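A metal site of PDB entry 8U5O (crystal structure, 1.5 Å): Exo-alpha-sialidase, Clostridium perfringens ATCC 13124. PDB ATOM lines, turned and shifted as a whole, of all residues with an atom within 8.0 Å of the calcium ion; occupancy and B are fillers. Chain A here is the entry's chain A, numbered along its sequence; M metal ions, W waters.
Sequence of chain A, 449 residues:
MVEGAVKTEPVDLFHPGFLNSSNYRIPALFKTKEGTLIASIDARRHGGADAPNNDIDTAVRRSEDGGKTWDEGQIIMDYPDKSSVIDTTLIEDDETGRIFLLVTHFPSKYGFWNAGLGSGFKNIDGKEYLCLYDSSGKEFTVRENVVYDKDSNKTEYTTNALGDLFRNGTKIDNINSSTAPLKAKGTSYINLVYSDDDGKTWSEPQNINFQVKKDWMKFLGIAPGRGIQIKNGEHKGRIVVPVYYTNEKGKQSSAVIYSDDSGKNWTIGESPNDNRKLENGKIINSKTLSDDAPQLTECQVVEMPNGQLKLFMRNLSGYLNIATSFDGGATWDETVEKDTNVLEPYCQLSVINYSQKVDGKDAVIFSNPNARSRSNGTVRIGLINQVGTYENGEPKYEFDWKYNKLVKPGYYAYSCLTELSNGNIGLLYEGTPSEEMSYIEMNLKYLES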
ATOM      1  N   ALA A  43     -12.101 -36.711 -11.101  1.00  0.00           N
ATOM      2  CA  ALA A  43     -12.220 -36.680 -12.560  1.00  0.00           C
ATOM      3  C   ALA A  43     -11.215 -35.645 -13.067  1.00  0.00           C
ATOM      4  O   ALA A  43     -11.420 -34.431 -12.935  1.00  0.00           O
ATOM      5  CB  ALA A  43     -13.661 -36.364 -12.946  1.00  0.00           C
ATOM      6  N   ARG A  45      -9.502 -33.761 -15.739  1.00  0.00           N
ATOM      7  CA  ARG A  45     -10.055 -33.502 -17.064  1.00  0.00           C
ATOM      8  C   ARG A  45      -9.009 -33.298 -18.157  1.00  0.00           C
ATOM      9  O   ARG A  45      -9.386 -33.336 -19.343  1.00  0.00           O
ATOM     10  CB  ARG A  45     -10.957 -32.277 -17.057  1.00  0.00           C
ATOM     11  CG  ARG A  45     -12.076 -32.309 -16.008  1.00  0.00           C
ATOM     12  CD  ARG A  45     -12.903 -33.592 -16.116  1.00  0.00           C
ATOM     13  NE  ARG A  45     -13.760 -33.633 -17.287  1.00  0.00           N
ATOM     14  CZ  ARG A  45     -14.974 -33.098 -17.335  1.00  0.00           C
ATOM     15  NH1 ARG A  45     -15.468 -32.421 -16.302  1.00  0.00           N
ATOM     16  NH2 ARG A  45     -15.702 -33.221 -18.451  1.00  0.00           N
ATOM     17  N   HIS A  46      -7.745 -33.054 -17.799  1.00  0.00           N
ATOM     18  CA  HIS A  46      -6.693 -32.753 -18.775  1.00  0.00           C
ATOM     19  C   HIS A  46      -5.453 -33.584 -18.518  1.00  0.00           C
ATOM     20  O   HIS A  46      -4.330 -33.077 -18.463  1.00  0.00           O
ATOM     21  CB  HIS A  46      -6.392 -31.263 -18.729  1.00  0.00           C
ATOM     22  CG  HIS A  46      -7.581 -30.432 -19.055  1.00  0.00           C
ATOM     23  ND1 HIS A  46      -8.228 -30.519 -20.274  1.00  0.00           N
ATOM     24  CD2 HIS A  46      -8.314 -29.581 -18.303  1.00  0.00           C
ATOM     25  CE1 HIS A  46      -9.276 -29.712 -20.265  1.00  0.00           C
ATOM     26  NE2 HIS A  46      -9.340 -29.119 -19.085  1.00  0.00           N
ATOM     27  N   ASN A  54      -3.735 -29.134 -14.077  1.00  0.00           N
ATOM     28  CA  ASN A  54      -4.934 -29.841 -14.482  1.00  0.00           C
ATOM     29  C   ASN A  54      -6.147 -29.003 -14.087  1.00  0.00           C
ATOM     30  O   ASN A  54      -6.039 -27.907 -13.524  1.00  0.00           O
ATOM     31  CB  ASN A  54      -4.980 -31.191 -13.767  1.00  0.00           C
ATOM     32  CG  ASN A  54      -5.586 -32.290 -14.621  1.00  0.00           C
ATOM     33  OD1 ASN A  54      -6.538 -32.059 -15.356  1.00  0.00           O
ATOM     34  ND2 ASN A  54      -5.043 -33.485 -14.498  1.00  0.00           N
ATOM     35  N   ASP A  55      -7.320 -29.559 -14.386  1.00  0.00           N
ATOM     36  CA  ASP A  55      -8.588 -29.031 -13.921  1.00  0.00           C
ATOM     37  C   ASP A  55      -9.336 -30.272 -13.474  1.00  0.00           C
ATOM     38  O   ASP A  55      -9.711 -31.100 -14.298  1.00  0.00           O
ATOM     39  CB  ASP A  55      -9.316 -28.325 -15.068  1.00  0.00           C
ATOM     40  CG  ASP A  55     -10.508 -27.505 -14.597  1.00  0.00           C
ATOM     41  OD1 ASP A  55     -11.227 -27.972 -13.678  1.00  0.00           O
ATOM     42  OD2 ASP A  55     -10.719 -26.378 -15.162  1.00  0.00           O
ATOM     43  N   ILE A  56      -9.493 -30.419 -12.150  1.00  0.00           N
ATOM     44  CA  ILE A  56      -9.969 -31.660 -11.536  1.00  0.00           C
ATOM     45  C   ILE A  56     -11.292 -31.396 -10.839  1.00  0.00           C
ATOM     46  O   ILE A  56     -11.408 -30.443 -10.047  1.00  0.00           O
ATOM     47  CB  ILE A  56      -8.924 -32.221 -10.568  1.00  0.00           C
ATOM     48  CG1 ILE A  56      -7.584 -32.362 -11.297  1.00  0.00           C
ATOM     49  CG2 ILE A  56      -9.464 -33.559 -10.046  1.00  0.00           C
ATOM     50  CD1 ILE A  56      -6.423 -32.741 -10.422  1.00  0.00           C
ATOM     51  N   ASP A  57     -12.289 -32.252 -11.124  1.00  0.00           N
ATOM     52  CA  ASP A  57     -13.614 -32.202 -10.515  1.00  0.00           C
ATOM     53  C   ASP A  57     -13.836 -33.459  -9.679  1.00  0.00           C
ATOM     54  O   ASP A  57     -13.150 -34.472  -9.861  1.00  0.00           O
ATOM     55  CB  ASP A  57     -14.694 -32.135 -11.614  1.00  0.00           C
ATOM     56  CG  ASP A  57     -14.426 -31.038 -12.623  1.00  0.00           C
ATOM     57  OD1 ASP A  57     -14.054 -29.926 -12.215  1.00  0.00           O
ATOM     58  OD2 ASP A  57     -14.640 -31.303 -13.848  1.00  0.00           O
ATOM     59  N   THR A  58     -14.790 -33.427  -8.760  1.00  0.00           N
ATOM     60  CA  THR A  58     -15.131 -34.593  -7.953  1.00  0.00           C
ATOM     61  C   THR A  58     -16.327 -35.317  -8.562  1.00  0.00           C
ATOM     62  O   THR A  58     -17.378 -34.709  -8.782  1.00  0.00           O
ATOM     63  CB  THR A  58     -15.533 -34.183  -6.540  1.00  0.00           C
ATOM     64  OG1 THR A  58     -14.444 -33.488  -5.909  1.00  0.00           O
ATOM     65  CG2 THR A  58     -15.875 -35.440  -5.711  1.00  0.00           C
ATOM     66  N   ILE A  75     -21.026 -35.348 -11.309  1.00  0.00           N
ATOM     67  CA  ILE A  75     -19.992 -34.429 -10.827  1.00  0.00           C
ATOM     68  C   ILE A  75     -20.621 -33.611  -9.714  1.00  0.00           C
ATOM     69  O   ILE A  75     -21.699 -33.015  -9.911  1.00  0.00           O
ATOM     70  CB  ILE A  75     -19.535 -33.510 -11.959  1.00  0.00           C
ATOM     71  CG1 ILE A  75     -18.987 -34.337 -13.115  1.00  0.00           C
ATOM     72  CG2 ILE A  75     -18.523 -32.479 -11.425  1.00  0.00           C
ATOM     73  CD1 ILE A  75     -17.795 -35.161 -12.752  1.00  0.00           C
ATOM     74  N   MET A  77     -18.547 -31.478  -7.395  1.00  0.00           N
ATOM     75  CA  MET A  77     -17.784 -30.242  -7.285  1.00  0.00           C
ATOM     76  C   MET A  77     -16.974 -29.943  -8.529  1.00  0.00           C
ATOM     77  O   MET A  77     -16.277 -30.825  -9.048  1.00  0.00           O
ATOM     78  CB  MET A  77     -16.910 -30.029  -6.018  1.00  0.00           C
ATOM     79  CG  MET A  77     -17.654 -30.128  -4.709  1.00  0.00           C
ATOM     80  SD  MET A  77     -16.546 -30.174  -3.284  1.00  0.00           S
ATOM     81  CE  MET A  77     -16.459 -31.971  -3.162  1.00  0.00           C
ATOM     82  N   ASP A  78     -17.066 -28.703  -9.005  1.00  0.00           N
ATOM     83  CA  ASP A  78     -16.429 -28.306 -10.251  1.00  0.00           C
ATOM     84  C   ASP A  78     -16.182 -26.813 -10.111  1.00  0.00           C
ATOM     85  O   ASP A  78     -17.155 -26.033 -10.053  1.00  0.00           O
ATOM     86  CB  ASP A  78     -17.375 -28.603 -11.419  1.00  0.00           C
ATOM     87  CG  ASP A  78     -16.838 -28.131 -12.753  1.00  0.00           C
ATOM     88  OD1 ASP A  78     -15.777 -27.481 -12.817  1.00  0.00           O
ATOM     89  OD2 ASP A  78     -17.507 -28.417 -13.782  1.00  0.00           O
ATOM     90  N   TYR A  79     -14.920 -26.439  -9.972  1.00  0.00           N
ATOM     91  CA  TYR A  79     -14.502 -25.040  -9.999  1.00  0.00           C
ATOM     92  C   TYR A  79     -13.910 -24.713 -11.363  1.00  0.00           C
ATOM     93  O   TYR A  79     -13.453 -25.607 -12.075  1.00  0.00           O
ATOM     94  CB  TYR A  79     -13.471 -24.791  -8.898  1.00  0.00           C
ATOM     95  CG  TYR A  79     -13.984 -24.880  -7.487  1.00  0.00           C
ATOM     96  CD1 TYR A  79     -13.984 -26.090  -6.791  1.00  0.00           C
ATOM     97  CD2 TYR A  79     -14.510 -23.760  -6.838  1.00  0.00           C
ATOM     98  CE1 TYR A  79     -14.420 -26.135  -5.466  1.00  0.00           C
ATOM     99  CE2 TYR A  79     -14.947 -23.816  -5.542  1.00  0.00           C
ATOM    100  CZ  TYR A  79     -14.911 -25.002  -4.852  1.00  0.00           C
ATOM    101  OH  TYR A  79     -15.348 -25.012  -3.555  1.00  0.00           O
ATOM    102  N   PRO A  80     -13.898 -23.449 -11.770  1.00  0.00           N
ATOM    103  CA  PRO A  80     -13.527 -23.129 -13.145  1.00  0.00           C
ATOM    104  C   PRO A  80     -12.022 -22.911 -13.302  1.00  0.00           C
ATOM    105  O   PRO A  80     -11.289 -22.737 -12.333  1.00  0.00           O
ATOM    106  CB  PRO A  80     -14.264 -21.800 -13.385  1.00  0.00           C
ATOM    107  CG  PRO A  80     -14.319 -21.174 -12.075  1.00  0.00           C
ATOM    108  CD  PRO A  80     -14.514 -22.301 -11.086  1.00  0.00           C
ATOM    109  N   ASP A  81     -11.597 -22.956 -14.568  1.00  0.00           N
ATOM    110  CA  ASP A  81     -10.311 -22.366 -14.977  1.00  0.00           C
ATOM    111  C   ASP A  81      -9.119 -22.916 -14.185  1.00  0.00           C
ATOM    112  O   ASP A  81      -8.266 -22.167 -13.716  1.00  0.00           O
ATOM    113  CB  ASP A  81     -10.392 -20.841 -14.872  1.00  0.00           C
ATOM    114  CG  ASP A  81      -9.202 -20.138 -15.512  1.00  0.00           C
ATOM    115  OD1 ASP A  81      -8.530 -20.729 -16.391  1.00  0.00           O
ATOM    116  OD2 ASP A  81      -8.945 -18.990 -15.116  1.00  0.00           O
ATOM    117  N   LYS A  82      -9.061 -24.238 -14.076  1.00  0.00           N
ATOM    118  CA  LYS A  82      -7.924 -24.951 -13.471  1.00  0.00           C
ATOM    119  C   LYS A  82      -7.836 -24.763 -11.960  1.00  0.00           C
ATOM    120  O   LYS A  82      -6.789 -25.020 -11.376  1.00  0.00           O
ATOM    121  CB  LYS A  82      -6.569 -24.676 -14.139  1.00  0.00           C
ATOM    122  CG  LYS A  82      -6.590 -25.054 -15.613  1.00  0.00           C
ATOM    123  CD  LYS A  82      -5.266 -24.688 -16.306  1.00  0.00           C
ATOM    124  CE  LYS A  82      -4.155 -25.666 -15.890  1.00  0.00           C
ATOM    125  NZ  LYS A  82      -2.849 -25.245 -16.482  1.00  0.00           N
ATOM    126  N   SER A  83      -8.932 -24.347 -11.328  1.00  0.00           N
ATOM    127  CA  SER A  83      -9.055 -24.509  -9.893  1.00  0.00           C
ATOM    128  C   SER A  83      -9.550 -25.932  -9.666  1.00  0.00           C
ATOM    129  O   SER A  83     -10.559 -26.331 -10.253  1.00  0.00           O
ATOM    130  CB  SER A  83     -10.060 -23.504  -9.345  1.00  0.00           C
ATOM    131  OG  SER A  83     -10.312 -23.706  -7.947  1.00  0.00           O
ATOM    132  N   SER A  84      -8.830 -26.696  -8.856  1.00  0.00           N
ATOM    133  CA  SER A  84      -9.124 -28.128  -8.725  1.00  0.00           C
ATOM    134  C   SER A  84      -9.582 -28.513  -7.341  1.00  0.00           C
ATOM    135  O   SER A  84      -9.200 -27.895  -6.328  1.00  0.00           O
ATOM    136  CB  SER A  84      -7.869 -28.932  -9.019  1.00  0.00           C
ATOM    137  OG  SER A  84      -7.592 -28.959 -10.414  1.00  0.00           O
ATOM    138  N   VAL A  85     -10.411 -29.549  -7.298  1.00  0.00           N
ATOM    139  CA  VAL A  85     -10.684 -30.309  -6.080  1.00  0.00           C
ATOM    140  C   VAL A  85     -10.015 -31.669  -6.242  1.00  0.00           C
ATOM    141  O   VAL A  85     -10.228 -32.362  -7.251  1.00  0.00           O
ATOM    142  CB  VAL A  85     -12.189 -30.450  -5.781  1.00  0.00           C
ATOM    143  CG1 VAL A  85     -12.706 -29.170  -5.085  1.00  0.00           C
ATOM    144  CG2 VAL A  85     -12.989 -30.710  -7.054  1.00  0.00           C
HETATM  145 CA    CA M   1     -13.472 -27.778 -13.074  1.00  0.00          CA
HETATM  146  O   HOH W   1     -14.001 -29.103 -15.117  1.00  0.00           O
HETATM  147  O   HOH W   2     -13.486 -26.219 -14.964  1.00  0.00           O
HETATM  148  O   HOH W   3     -12.557 -28.056 -10.762  1.00  0.00           O
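The backbone carbonyl oxygen (O) of Asp 55 sits at hydrogen-bond distance from the backbone NH (N) of Arg 45, at 3.0 Å. OD2 of Asp 55 sits at hydrogen-bond distance from N of Lys 82 (2.9 Å). OD2 of Asp 57 lies within salt-bridge range of NH1 of Arg 45, at 2.8 Å. O of Asp 57 lies within hydrogen-bond range of N of Ala 43.
Of the 18 residues printed, 4 come within 4 Å of the calcium ion. The nearest printed residue that does not touch the calcium ion is Ser 83 (4.3 Å).
The calcium ion is bound by OD1 of Asp 55 (2.3 Å), OD1 of Asp 78 (2.3 Å), OD1 of Asp 57 (2.4 Å), O of Tyr 79 (2.4 Å), water W2 (2.5 Å), water W1 (2.5 Å) and water W3 (2.5 Å).
Water W3 lies within hydrogen-bond range of the backbone carbonyl oxygen (O) of Ser 83 (2.7 Å), the backbone carbonyl oxygen (O) of Ile 56 (2.7 Å) and the backbone NH (N) of Tyr 79 (3.0 Å).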
